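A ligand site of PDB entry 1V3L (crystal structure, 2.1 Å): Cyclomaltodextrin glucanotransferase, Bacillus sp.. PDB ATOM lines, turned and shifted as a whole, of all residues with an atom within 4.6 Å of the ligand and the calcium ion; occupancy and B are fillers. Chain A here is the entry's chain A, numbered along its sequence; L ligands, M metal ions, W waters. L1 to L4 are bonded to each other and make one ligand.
The side-chain hydroxyl (OH) of Tyr 195 lies close to an oxygen (O6) of LIG L1, at 3.2 Å. The backbone carbonyl oxygen (O) of Glu 257 is in hydrogen-bond range of an oxygen (O2) of LG2 L2 (3.3 Å). The indole nitrogen of Trp 101 sits at hydrogen-bond distance from an oxygen (O5) of LG4 L4, at 2.7 Å. NE2 of His 233 is in hydrogen-bond range of O3 of LG2 L2 (3.5 Å). OD1 of Asp 371 is in hydrogen-bond range of O2 of LG4 L4, at 2.8 Å. An oxygen (O1) of LG3 L3 is in hydrogen-bond range of the side-chain carboxylate (OD2) of Asp 328 (2.7 Å). A ring nitrogen (NE2) of His 327 sits at hydrogen-bond distance from an oxygen (O1) of LG3 L3 (3.1 Å). An oxygen (O1) of LG2 L2 sits at hydrogen-bond distance from the backbone NH of Phe 259 (2.9 Å). NH2 of Arg 375 sits at hydrogen-bond distance from O1 of LG4 L4, at 3.0 Å.
Merely in contact with the ligand: His 98 (3.7 Å), Tyr 100 (3.7 Å), His 140 (3.7 Å), Leu 194 (3.7 Å), Leu 197 (3.4 Å), Asp 229 (3.2 Å), Lys 232 (3.7 Å) and Trp 258 (3.98 Å). Hydrophobic or aromatic side chains within 4 Å of the ligand: His 98, Tyr 100, Trp 101, His 140, Leu 194, Tyr 195, Leu 197, Phe 259 and His 327. Along chain A the residues within 4 Å of the ligand span positions 98 to 375. The nearest printed residue that does not touch the ligand is Tyr 97 (4.1 Å).
Water W7 lies within hydrogen-bond range of an oxygen (O2) of LG2 L2 (2.6 Å), the backbone NH of Ala 230 (2.8 Å) and the side-chain carboxylate of Asp 229 (3.3 Å). Water W3 lies within hydrogen-bond range of O2 of LG2 L2 (2.6 Å), O of Glu 257 (2.8 Å) and N of Lys 232 (3.0 Å). Water W6 lies within hydrogen-bond range of the side-chain hydroxyl of Tyr 97 (2.7 Å), the side-chain carboxylate of Asp 371 (2.8 Å) and an oxygen (O2) of LG4 L4 (3.1 Å).
Of the 27 residues printed, 4 come within 4 Å of the calcium ion.
The calcium ion is bound by water W1, 2.2 Å away. O of Ile 190 binds the calcium ion. Water W2 is bound to the calcium ion, 2.3 Å away. The backbone carbonyl oxygen (O) of His 233 binds the calcium ion (2.4 Å). The calcium ion is bound by water W4 (2.5 Å). The calcium ion is bound by OD1 of Asp 199 (2.6 Å). The calcium ion is bound by ND2 of Asn 139 (2.7 Å). OD2 of Asp 199 binds the calcium ion, 2.8 Å away.
The backbone carbonyl oxygen of His 327 is in hydrogen-bond range of the guanidinium group of Arg 375, 3.2 Å away. The guanidinium group (NH1) of Arg 375 lies within hydrogen-bond range of the side-chain hydroxyl (OH) of Tyr 97. The backbone carbonyl oxygen (O) of Phe 259 sits at hydrogen-bond distance from the side-chain amino group (NZ) of Lys 232 (3.2 Å). ND1 of His 233 is in hydrogen-bond range of O of Gly 189, 3.0 Å away. NH1 of Arg 375 is in salt-bridge range of OD2 of Asp 371. The backbone carbonyl oxygen (O) of Tyr 100 lies within hydrogen-bond range of a ring nitrogen (NE2) of His 140, 3.0 Å away. The side-chain amide oxygen (OD1) of Asn 139 is in hydrogen-bond range of a ring nitrogen (ND1) of His 140, at 3.0 Å. The backbone NH (N) of Tyr 100 sits close to a ring nitrogen (ND1) of His 98 (3.3 Å).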
ATOM      1  N   TYR A  97      -2.922  34.701  -5.417  1.00  0.00           N
ATOM      2  CA  TYR A  97      -3.906  34.825  -6.511  1.00  0.00           C
ATOM      3  C   TYR A  97      -4.432  33.482  -7.015  1.00  0.00           C
ATOM      4  O   TYR A  97      -5.569  33.389  -7.435  1.00  0.00           O
ATOM      5  CB  TYR A  97      -3.313  35.580  -7.720  1.00  0.00           C
ATOM      6  CG  TYR A  97      -2.267  34.825  -8.522  1.00  0.00           C
ATOM      7  CD1 TYR A  97      -2.652  34.039  -9.618  1.00  0.00           C
ATOM      8  CD2 TYR A  97      -0.920  34.894  -8.166  1.00  0.00           C
ATOM      9  CE1 TYR A  97      -1.710  33.331 -10.357  1.00  0.00           C
ATOM     10  CE2 TYR A  97       0.030  34.192  -8.905  1.00  0.00           C
ATOM     11  CZ  TYR A  97      -0.377  33.401  -9.980  1.00  0.00           C
ATOM     12  OH  TYR A  97       0.564  32.641 -10.651  1.00  0.00           O
ATOM     13  N   HIS A  98      -3.511  32.522  -7.003  1.00  0.00           N
ATOM     14  CA  HIS A  98      -3.657  31.115  -7.384  1.00  0.00           C
ATOM     15  C   HIS A  98      -4.450  30.213  -6.438  1.00  0.00           C
ATOM     16  O   HIS A  98      -4.820  29.102  -6.815  1.00  0.00           O
ATOM     17  CB  HIS A  98      -2.260  30.508  -7.595  1.00  0.00           C
ATOM     18  CG  HIS A  98      -1.223  30.682  -6.480  1.00  0.00           C
ATOM     19  ND1 HIS A  98      -1.256  30.455  -5.167  1.00  0.00           N
ATOM     20  CD2 HIS A  98       0.028  31.174  -6.757  1.00  0.00           C
ATOM     21  CE1 HIS A  98      -0.081  30.812  -4.678  1.00  0.00           C
ATOM     22  NE2 HIS A  98       0.699  31.247  -5.632  1.00  0.00           N
ATOM     23  N   TYR A 100      -3.538  28.462  -3.803  1.00  0.00           N
ATOM     24  CA  TYR A 100      -2.806  27.325  -3.254  1.00  0.00           C
ATOM     25  C   TYR A 100      -2.185  27.521  -1.864  1.00  0.00           C
ATOM     26  O   TYR A 100      -1.574  26.583  -1.376  1.00  0.00           O
ATOM     27  CB  TYR A 100      -1.651  26.915  -4.195  1.00  0.00           C
ATOM     28  CG  TYR A 100      -2.027  26.389  -5.591  1.00  0.00           C
ATOM     29  CD1 TYR A 100      -2.832  25.239  -5.705  1.00  0.00           C
ATOM     30  CD2 TYR A 100      -1.550  27.029  -6.764  1.00  0.00           C
ATOM     31  CE1 TYR A 100      -3.153  24.719  -6.961  1.00  0.00           C
ATOM     32  CE2 TYR A 100      -1.863  26.515  -8.030  1.00  0.00           C
ATOM     33  CZ  TYR A 100      -2.662  25.355  -8.114  1.00  0.00           C
ATOM     34  OH  TYR A 100      -3.008  24.818  -9.341  1.00  0.00           O
ATOM     35  N   TRP A 101      -2.268  28.692  -1.258  1.00  0.00           N
ATOM     36  CA  TRP A 101      -1.627  28.968  -0.004  1.00  0.00           C
ATOM     37  C   TRP A 101      -2.772  29.058   0.984  1.00  0.00           C
ATOM     38  O   TRP A 101      -3.156  30.142   1.420  1.00  0.00           O
ATOM     39  CB  TRP A 101      -0.901  30.258  -0.145  1.00  0.00           C
ATOM     40  CG  TRP A 101       0.357  30.214  -1.003  1.00  0.00           C
ATOM     41  CD1 TRP A 101       0.910  29.039  -1.454  1.00  0.00           C
ATOM     42  CD2 TRP A 101       1.112  31.303  -1.351  1.00  0.00           C
ATOM     43  NE1 TRP A 101       2.036  29.402  -2.075  1.00  0.00           N
ATOM     44  CE2 TRP A 101       2.181  30.727  -2.037  1.00  0.00           C
ATOM     45  CE3 TRP A 101       1.053  32.679  -1.178  1.00  0.00           C
ATOM     46  CZ2 TRP A 101       3.210  31.502  -2.550  1.00  0.00           C
ATOM     47  CZ3 TRP A 101       2.090  33.459  -1.692  1.00  0.00           C
ATOM     48  CH2 TRP A 101       3.152  32.877  -2.378  1.00  0.00           C
ATOM     49  N   ASN A 139      -2.413  19.174   0.946  1.00  0.00           N
ATOM     50  CA  ASN A 139      -1.060  18.803   1.266  1.00  0.00           C
ATOM     51  C   ASN A 139      -0.356  19.762   2.224  1.00  0.00           C
ATOM     52  O   ASN A 139       0.512  19.333   2.988  1.00  0.00           O
ATOM     53  CB  ASN A 139      -0.274  18.714  -0.008  1.00  0.00           C
ATOM     54  CG  ASN A 139       1.193  18.499   0.146  1.00  0.00           C
ATOM     55  OD1 ASN A 139       1.992  19.396  -0.100  1.00  0.00           O
ATOM     56  ND2 ASN A 139       1.713  17.358   0.567  1.00  0.00           N
ATOM     57  N   HIS A 140      -0.712  21.030   2.207  1.00  0.00           N
ATOM     58  CA  HIS A 140       0.027  22.050   2.896  1.00  0.00           C
ATOM     59  C   HIS A 140      -0.889  23.196   3.131  1.00  0.00           C
ATOM     60  O   HIS A 140      -1.989  23.230   2.566  1.00  0.00           O
ATOM     61  CB  HIS A 140       1.230  22.463   2.037  1.00  0.00           C
ATOM     62  CG  HIS A 140       0.821  22.903   0.647  1.00  0.00           C
ATOM     63  ND1 HIS A 140       0.818  22.157  -0.462  1.00  0.00           N
ATOM     64  CD2 HIS A 140       0.300  24.134   0.350  1.00  0.00           C
ATOM     65  CE1 HIS A 140       0.275  22.896  -1.398  1.00  0.00           C
ATOM     66  NE2 HIS A 140      -0.031  24.078  -0.899  1.00  0.00           N
ATOM     67  N   HIS A 176       4.763  18.620   9.274  1.00  0.00           N
ATOM     68  CA  HIS A 176       6.013  17.872   9.200  1.00  0.00           C
ATOM     69  C   HIS A 176       7.166  18.807   9.361  1.00  0.00           C
ATOM     70  O   HIS A 176       7.109  19.960   8.885  1.00  0.00           O
ATOM     71  CB  HIS A 176       6.340  17.212   7.870  1.00  0.00           C
ATOM     72  CG  HIS A 176       5.428  16.083   7.558  1.00  0.00           C
ATOM     73  ND1 HIS A 176       5.000  15.864   6.345  1.00  0.00           N
ATOM     74  CD2 HIS A 176       4.856  15.178   8.422  1.00  0.00           C
ATOM     75  CE1 HIS A 176       4.148  14.854   6.427  1.00  0.00           C
ATOM     76  NE2 HIS A 176       4.078  14.449   7.674  1.00  0.00           N
ATOM     77  N   GLY A 189       9.781  13.211  -1.140  1.00  0.00           N
ATOM     78  CA  GLY A 189       8.851  14.246  -1.560  1.00  0.00           C
ATOM     79  C   GLY A 189       7.526  14.249  -0.803  1.00  0.00           C
ATOM     80  O   GLY A 189       6.792  15.254  -0.876  1.00  0.00           O
ATOM     81  N   ILE A 190       7.198  13.198  -0.048  1.00  0.00           N
ATOM     82  CA  ILE A 190       5.931  13.097   0.694  1.00  0.00           C
ATOM     83  C   ILE A 190       6.004  13.734   2.068  1.00  0.00           C
ATOM     84  O   ILE A 190       5.077  14.516   2.450  1.00  0.00           O
ATOM     85  CB  ILE A 190       5.500  11.619   0.854  1.00  0.00           C
ATOM     86  CG1 ILE A 190       5.177  11.068  -0.534  1.00  0.00           C
ATOM     87  CG2 ILE A 190       4.291  11.500   1.755  1.00  0.00           C
ATOM     88  CD1 ILE A 190       4.876   9.579  -0.607  1.00  0.00           C
ATOM     89  N   TYR A 191       7.076  13.396   2.793  1.00  0.00           N
ATOM     90  CA  TYR A 191       7.220  13.801   4.188  1.00  0.00           C
ATOM     91  C   TYR A 191       8.028  15.070   4.386  1.00  0.00           C
ATOM     92  O   TYR A 191       7.782  15.739   5.395  1.00  0.00           O
ATOM     93  CB  TYR A 191       7.814  12.630   5.037  1.00  0.00           C
ATOM     94  CG  TYR A 191       6.880  11.402   5.012  1.00  0.00           C
ATOM     95  CD1 TYR A 191       5.645  11.508   5.632  1.00  0.00           C
ATOM     96  CD2 TYR A 191       7.208  10.244   4.304  1.00  0.00           C
ATOM     97  CE1 TYR A 191       4.726  10.473   5.554  1.00  0.00           C
ATOM     98  CE2 TYR A 191       6.273   9.199   4.206  1.00  0.00           C
ATOM     99  CZ  TYR A 191       5.052   9.338   4.836  1.00  0.00           C
ATOM    100  OH  TYR A 191       4.115   8.312   4.809  1.00  0.00           O
ATOM    101  N   LYS A 192       8.821  15.468   3.410  1.00  0.00           N
ATOM    102  CA  LYS A 192       9.473  16.756   3.511  1.00  0.00           C
ATOM    103  C   LYS A 192       8.634  17.840   2.832  1.00  0.00           C
ATOM    104  O   LYS A 192       7.658  17.567   2.123  1.00  0.00           O
ATOM    105  CB  LYS A 192      10.847  16.696   2.871  1.00  0.00           C
ATOM    106  CG  LYS A 192      11.746  15.665   3.552  1.00  0.00           C
ATOM    107  CD  LYS A 192      13.197  15.932   3.214  1.00  0.00           C
ATOM    108  CE  LYS A 192      14.100  15.019   4.009  1.00  0.00           C
ATOM    109  NZ  LYS A 192      15.468  15.305   3.622  1.00  0.00           N
ATOM    110  N   LEU A 194       7.473  20.876   0.318  1.00  0.00           N
ATOM    111  CA  LEU A 194       7.668  21.241  -1.091  1.00  0.00           C
ATOM    112  C   LEU A 194       7.988  22.718  -1.019  1.00  0.00           C
ATOM    113  O   LEU A 194       7.194  23.551  -0.578  1.00  0.00           O
ATOM    114  CB  LEU A 194       6.422  21.088  -2.063  1.00  0.00           C
ATOM    115  CG  LEU A 194       4.986  20.708  -1.669  1.00  0.00           C
ATOM    116  CD1 LEU A 194       4.014  20.833  -2.843  1.00  0.00           C
ATOM    117  CD2 LEU A 194       4.977  19.260  -1.243  1.00  0.00           C
ATOM    118  N   TYR A 195       9.225  23.037  -1.413  1.00  0.00           N
ATOM    119  CA  TYR A 195       9.758  24.396  -1.428  1.00  0.00           C
ATOM    120  C   TYR A 195       9.702  24.882   0.022  1.00  0.00           C
ATOM    121  O   TYR A 195      10.394  24.320   0.863  1.00  0.00           O
ATOM    122  CB  TYR A 195       8.911  25.318  -2.384  1.00  0.00           C
ATOM    123  CG  TYR A 195       8.287  24.692  -3.651  1.00  0.00           C
ATOM    124  CD1 TYR A 195       9.067  24.215  -4.709  1.00  0.00           C
ATOM    125  CD2 TYR A 195       6.889  24.625  -3.746  1.00  0.00           C
ATOM    126  CE1 TYR A 195       8.461  23.668  -5.853  1.00  0.00           C
ATOM    127  CE2 TYR A 195       6.283  24.078  -4.880  1.00  0.00           C
ATOM    128  CZ  TYR A 195       7.071  23.606  -5.929  1.00  0.00           C
ATOM    129  OH  TYR A 195       6.445  23.106  -7.071  1.00  0.00           O
ATOM    130  N   LEU A 197       6.525  25.420   1.713  1.00  0.00           N
ATOM    131  CA  LEU A 197       5.129  25.322   2.046  1.00  0.00           C
ATOM    132  C   LEU A 197       5.022  24.470   3.287  1.00  0.00           C
ATOM    133  O   LEU A 197       5.578  23.372   3.298  1.00  0.00           O
ATOM    134  CB  LEU A 197       4.385  24.695   0.881  1.00  0.00           C
ATOM    135  CG  LEU A 197       4.394  25.426  -0.453  1.00  0.00           C
ATOM    136  CD1 LEU A 197       3.746  24.581  -1.517  1.00  0.00           C
ATOM    137  CD2 LEU A 197       3.667  26.739  -0.304  1.00  0.00           C
ATOM    138  N   ASP A 199       4.099  21.770   5.258  1.00  0.00           N
ATOM    139  CA  ASP A 199       3.567  20.449   4.994  1.00  0.00           C
ATOM    140  C   ASP A 199       2.609  19.901   6.056  1.00  0.00           C
ATOM    141  O   ASP A 199       3.036  19.619   7.171  1.00  0.00           O
ATOM    142  CB  ASP A 199       4.756  19.507   4.824  1.00  0.00           C
ATOM    143  CG  ASP A 199       4.544  18.462   3.736  1.00  0.00           C
ATOM    144  OD1 ASP A 199       4.897  17.303   3.958  1.00  0.00           O
ATOM    145  OD2 ASP A 199       3.991  18.803   2.685  1.00  0.00           O
ATOM    146  N   ASP A 229      -4.839  18.480  -5.475  1.00  0.00           N
ATOM    147  CA  ASP A 229      -3.529  18.975  -5.783  1.00  0.00           C
ATOM    148  C   ASP A 229      -2.521  18.158  -5.015  1.00  0.00           C
ATOM    149  O   ASP A 229      -2.770  17.735  -3.887  1.00  0.00           O
ATOM    150  CB  ASP A 229      -3.435  20.442  -5.358  1.00  0.00           C
ATOM    151  CG  ASP A 229      -2.144  21.182  -5.756  1.00  0.00           C
ATOM    152  OD1 ASP A 229      -2.032  21.505  -6.936  1.00  0.00           O
ATOM    153  OD2 ASP A 229      -1.261  21.411  -4.898  1.00  0.00           O
ATOM    154  N   ALA A 230      -1.319  18.100  -5.583  1.00  0.00           N
ATOM    155  CA  ALA A 230      -0.123  17.422  -5.103  1.00  0.00           C
ATOM    156  C   ALA A 230      -0.237  15.983  -4.555  1.00  0.00           C
ATOM    157  O   ALA A 230       0.401  15.571  -3.588  1.00  0.00           O
ATOM    158  CB  ALA A 230       0.530  18.332  -4.066  1.00  0.00           C
ATOM    159  N   LYS A 232       1.213  13.411  -5.571  1.00  0.00           N
ATOM    160  CA  LYS A 232       2.534  12.789  -5.520  1.00  0.00           C
ATOM    161  C   LYS A 232       3.261  13.097  -4.217  1.00  0.00           C
ATOM    162  O   LYS A 232       4.343  12.556  -3.930  1.00  0.00           O
ATOM    163  CB  LYS A 232       3.321  13.325  -6.731  1.00  0.00           C
ATOM    164  CG  LYS A 232       4.606  12.603  -7.114  1.00  0.00           C
ATOM    165  CD  LYS A 232       5.380  13.283  -8.249  1.00  0.00           C
ATOM    166  CE  LYS A 232       6.606  12.397  -8.558  1.00  0.00           C
ATOM    167  NZ  LYS A 232       7.412  12.904  -9.659  1.00  0.00           N
ATOM    168  N   HIS A 233       2.708  14.014  -3.415  1.00  0.00           N
ATOM    169  CA  HIS A 233       3.359  14.492  -2.204  1.00  0.00           C
ATOM    170  C   HIS A 233       2.629  14.207  -0.894  1.00  0.00           C
ATOM    171  O   HIS A 233       2.962  14.804   0.165  1.00  0.00           O
ATOM    172  CB  HIS A 233       3.592  15.996  -2.400  1.00  0.00           C
ATOM    173  CG  HIS A 233       4.582  16.230  -3.514  1.00  0.00           C
ATOM    174  ND1 HIS A 233       5.814  15.725  -3.629  1.00  0.00           N
ATOM    175  CD2 HIS A 233       4.330  16.969  -4.644  1.00  0.00           C
ATOM    176  CE1 HIS A 233       6.306  16.108  -4.771  1.00  0.00           C
ATOM    177  NE2 HIS A 233       5.403  16.855  -5.362  1.00  0.00           N
ATOM    178  N   MET A 234       1.651  13.297  -0.907  1.00  0.00           N
ATOM    179  CA  MET A 234       0.864  12.921   0.250  1.00  0.00           C
ATOM    180  C   MET A 234       0.881  11.423   0.293  1.00  0.00           C
ATOM    181  O   MET A 234       1.048  10.800  -0.763  1.00  0.00           O
ATOM    182  CB  MET A 234      -0.592  13.370   0.144  1.00  0.00           C
ATOM    183  CG  MET A 234      -0.788  14.863   0.213  1.00  0.00           C
ATOM    184  SD  MET A 234      -2.545  15.276   0.170  1.00  0.00           S
ATOM    185  CE  MET A 234      -2.819  15.233  -1.579  1.00  0.00           C
ATOM    186  N   GLU A 257      -2.888  14.984 -10.275  1.00  0.00           N
ATOM    187  CA  GLU A 257      -1.807  15.043 -11.246  1.00  0.00           C
ATOM    188  C   GLU A 257      -0.575  14.328 -10.728  1.00  0.00           C
ATOM    189  O   GLU A 257      -0.010  14.831  -9.755  1.00  0.00           O
ATOM    190  CB  GLU A 257      -1.455  16.535 -11.535  1.00  0.00           C
ATOM    191  CG  GLU A 257      -0.276  16.913 -12.486  1.00  0.00           C
ATOM    192  CD  GLU A 257      -0.132  18.410 -12.801  1.00  0.00           C
ATOM    193  OE1 GLU A 257       0.344  18.744 -13.905  1.00  0.00           O
ATOM    194  OE2 GLU A 257      -0.469  19.254 -11.965  1.00  0.00           O
ATOM    195  N   TRP A 258      -0.131  13.191 -11.237  1.00  0.00           N
ATOM    196  CA  TRP A 258       1.160  12.676 -10.792  1.00  0.00           C
ATOM    197  C   TRP A 258       2.088  13.252 -11.872  1.00  0.00           C
ATOM    198  O   TRP A 258       1.909  12.860 -13.026  1.00  0.00           O
ATOM    199  CB  TRP A 258       1.093  11.161 -10.808  1.00  0.00           C
ATOM    200  CG  TRP A 258       2.323  10.430 -10.251  1.00  0.00           C
ATOM    201  CD1 TRP A 258       3.519  10.348 -10.929  1.00  0.00           C
ATOM    202  CD2 TRP A 258       2.376   9.771  -9.045  1.00  0.00           C
ATOM    203  NE1 TRP A 258       4.338   9.634 -10.175  1.00  0.00           N
ATOM    204  CE2 TRP A 258       3.698   9.273  -9.050  1.00  0.00           C
ATOM    205  CE3 TRP A 258       1.508   9.537  -7.982  1.00  0.00           C
ATOM    206  CZ2 TRP A 258       4.158   8.532  -7.973  1.00  0.00           C
ATOM    207  CZ3 TRP A 258       1.987   8.785  -6.906  1.00  0.00           C
ATOM    208  CH2 TRP A 258       3.295   8.289  -6.911  1.00  0.00           C
ATOM    209  N   PHE A 259       3.031  14.177 -11.659  1.00  0.00           N
ATOM    210  CA  PHE A 259       3.803  14.699 -12.790  1.00  0.00           C
ATOM    211  C   PHE A 259       4.919  13.744 -13.190  1.00  0.00           C
ATOM    212  O   PHE A 259       5.677  13.191 -12.389  1.00  0.00           O
ATOM    213  CB  PHE A 259       4.404  16.077 -12.465  1.00  0.00           C
ATOM    214  CG  PHE A 259       4.677  16.932 -13.707  1.00  0.00           C
ATOM    215  CD1 PHE A 259       3.692  17.834 -14.151  1.00  0.00           C
ATOM    216  CD2 PHE A 259       5.873  16.780 -14.428  1.00  0.00           C
ATOM    217  CE1 PHE A 259       3.903  18.583 -15.306  1.00  0.00           C
ATOM    218  CE2 PHE A 259       6.086  17.543 -15.593  1.00  0.00           C
ATOM    219  CZ  PHE A 259       5.093  18.439 -16.027  1.00  0.00           C
ATOM    220  N   HIS A 327      -1.842  25.029 -16.293  1.00  0.00           N
ATOM    221  CA  HIS A 327      -1.036  25.893 -15.440  1.00  0.00           C
ATOM    222  C   HIS A 327       0.427  25.539 -15.211  1.00  0.00           C
ATOM    223  O   HIS A 327       1.165  26.385 -14.708  1.00  0.00           O
ATOM    224  CB  HIS A 327      -1.758  26.010 -14.116  1.00  0.00           C
ATOM    225  CG  HIS A 327      -2.000  24.670 -13.433  1.00  0.00           C
ATOM    226  ND1 HIS A 327      -2.952  23.778 -13.695  1.00  0.00           N
ATOM    227  CD2 HIS A 327      -1.193  24.167 -12.451  1.00  0.00           C
ATOM    228  CE1 HIS A 327      -2.720  22.753 -12.906  1.00  0.00           C
ATOM    229  NE2 HIS A 327      -1.663  22.994 -12.169  1.00  0.00           N
ATOM    230  N   ASP A 328       0.866  24.316 -15.513  1.00  0.00           N
ATOM    231  CA  ASP A 328       2.222  23.851 -15.227  1.00  0.00           C
ATOM    232  C   ASP A 328       3.151  23.782 -16.392  1.00  0.00           C
ATOM    233  O   ASP A 328       4.294  23.314 -16.274  1.00  0.00           O
ATOM    234  CB  ASP A 328       2.179  22.467 -14.588  1.00  0.00           C
ATOM    235  CG  ASP A 328       1.853  22.458 -13.113  1.00  0.00           C
ATOM    236  OD1 ASP A 328       1.849  23.510 -12.463  1.00  0.00           O
ATOM    237  OD2 ASP A 328       1.641  21.363 -12.592  1.00  0.00           O
ATOM    238  N   ASP A 371       5.019  29.329 -15.625  1.00  0.00           N
ATOM    239  CA  ASP A 371       4.611  30.148 -14.488  1.00  0.00           C
ATOM    240  C   ASP A 371       5.543  31.338 -14.185  1.00  0.00           C
ATOM    241  O   ASP A 371       6.752  31.167 -14.036  1.00  0.00           O
ATOM    242  CB  ASP A 371       4.512  29.195 -13.312  1.00  0.00           C
ATOM    243  CG  ASP A 371       4.024  29.735 -11.985  1.00  0.00           C
ATOM    244  OD1 ASP A 371       4.250  29.057 -10.992  1.00  0.00           O
ATOM    245  OD2 ASP A 371       3.411  30.791 -11.927  1.00  0.00           O
ATOM    246  N   ARG A 375      -0.188  32.432 -17.075  1.00  0.00           N
ATOM    247  CA  ARG A 375      -1.403  32.775 -16.326  1.00  0.00           C
ATOM    248  C   ARG A 375      -1.804  34.237 -16.486  1.00  0.00           C
ATOM    249  O   ARG A 375      -2.317  34.875 -15.575  1.00  0.00           O
ATOM    250  CB  ARG A 375      -1.218  32.469 -14.839  1.00  0.00           C
ATOM    251  CG  ARG A 375      -1.012  30.990 -14.537  1.00  0.00           C
ATOM    252  CD  ARG A 375      -0.118  30.909 -13.330  1.00  0.00           C
ATOM    253  NE  ARG A 375       0.378  29.556 -13.117  1.00  0.00           N
ATOM    254  CZ  ARG A 375       0.636  29.023 -11.910  1.00  0.00           C
ATOM    255  NH1 ARG A 375       0.450  29.726 -10.790  1.00  0.00           N
ATOM    256  NH2 ARG A 375       1.112  27.772 -11.843  1.00  0.00           N
HETATM  257  C1  LIG L   1       6.857  20.931 -13.523  1.00  0.00           C
HETATM  258  C2  LIG L   1       7.850  20.311 -12.538  1.00  0.00           C
HETATM  259  C3  LIG L   1       7.075  19.348 -11.574  1.00  0.00           C
HETATM  260  C4  LIG L   1       5.833  20.000 -10.853  1.00  0.00           C
HETATM  261  C5  LIG L   1       5.058  21.030 -11.796  1.00  0.00           C
HETATM  262  C6  LIG L   1       4.466  22.183 -10.914  1.00  0.00           C
HETATM  263  O1  LIG L   1       7.656  21.679 -14.445  1.00  0.00           O
HETATM  264  O2  LIG L   1       8.915  19.599 -13.228  1.00  0.00           O
HETATM  265  O3  LIG L   1       7.990  18.951 -10.549  1.00  0.00           O
HETATM  266  O4  LIG L   1       4.901  18.957 -10.441  1.00  0.00           O
HETATM  267  O5  LIG L   1       5.906  21.741 -12.780  1.00  0.00           O
HETATM  268  O6  LIG L   1       5.465  22.741 -10.045  1.00  0.00           O
HETATM  269  C1  LG2 L   2       5.055  18.183  -9.181  1.00  0.00           C
HETATM  270  C2  LG2 L   2       3.755  17.406  -8.904  1.00  0.00           C
HETATM  271  C3  LG2 L   2       2.636  18.414  -9.172  1.00  0.00           C
HETATM  272  C4  LG2 L   2       2.701  19.552  -8.059  1.00  0.00           C
HETATM  273  C5  LG2 L   2       4.169  20.143  -7.875  1.00  0.00           C
HETATM  274  C6  LG2 L   2       4.457  20.817  -6.522  1.00  0.00           C
HETATM  275  O1  LG2 L   2       3.505  16.158  -9.558  1.00  0.00           O
HETATM  276  O2  LG2 L   2       1.379  17.740  -9.192  1.00  0.00           O
HETATM  277  O3  LG2 L   2       5.199  19.095  -8.027  1.00  0.00           O
HETATM  278  C1  LG3 L   3       1.060  21.563  -7.873  1.00  0.00           C
HETATM  279  C2  LG3 L   3       0.675  22.677  -8.887  1.00  0.00           C
HETATM  280  C3  LG3 L   3       1.731  23.831  -8.837  1.00  0.00           C
HETATM  281  C4  LG3 L   3       1.608  24.452  -7.370  1.00  0.00           C
HETATM  282  C5  LG3 L   3       1.797  23.394  -6.252  1.00  0.00           C
HETATM  283  C6  LG3 L   3       1.345  23.737  -4.842  1.00  0.00           C
HETATM  284  C7  LG3 L   3       1.674  22.023  -6.552  1.00  0.00           C
HETATM  285  N1  LG3 L   3       1.731  20.505  -8.612  1.00  0.00           N
HETATM  286  O1  LG3 L   3       0.619  22.159 -10.227  1.00  0.00           O
HETATM  287  O2  LG3 L   3       1.451  24.754  -9.929  1.00  0.00           O
HETATM  288  O3  LG3 L   3       2.603  25.495  -7.133  1.00  0.00           O
HETATM  289  O4  LG3 L   3       1.928  24.940  -4.394  1.00  0.00           O
HETATM  290  C1  LG4 L   4       2.113  26.717  -6.521  1.00  0.00           C
HETATM  291  C2  LG4 L   4       1.962  27.825  -7.658  1.00  0.00           C
HETATM  292  C3  LG4 L   4       3.208  28.718  -7.840  1.00  0.00           C
HETATM  293  C4  LG4 L   4       3.670  29.168  -6.407  1.00  0.00           C
HETATM  294  C5  LG4 L   4       4.155  27.822  -5.723  1.00  0.00           C
HETATM  295  C6  LG4 L   4       5.026  28.024  -4.456  1.00  0.00           C
HETATM  296  O1  LG4 L   4       1.732  27.223  -8.939  1.00  0.00           O
HETATM  297  O2  LG4 L   4       2.852  29.785  -8.696  1.00  0.00           O
HETATM  298  O3  LG4 L   4       4.637  30.203  -6.390  1.00  0.00           O
HETATM  299  O4  LG4 L   4       2.932  27.106  -5.385  1.00  0.00           O
HETATM  300  O5  LG4 L   4       4.146  28.545  -3.464  1.00  0.00           O
HETATM  301 CA    CA M   1       3.592  16.089   2.117  1.00  0.00          CA
HETATM  302  O   HOH W   1       5.230  16.847   0.925  1.00  0.00           O
HETATM  303  O   HOH W   2       1.913  16.878   3.449  1.00  0.00           O
HETATM  304  O   HOH W   3       1.436  15.666  -7.560  1.00  0.00           O
HETATM  305  O   HOH W   4       2.530  14.168   3.229  1.00  0.00           O
HETATM  306  O   HOH W   5       6.424  29.760  -2.406  1.00  0.00           O
HETATM  307  O   HOH W   6       3.148  32.650  -9.802  1.00  0.00           O
HETATM  308  O   HOH W   7      -0.807  18.771  -8.246  1.00  0.00           O
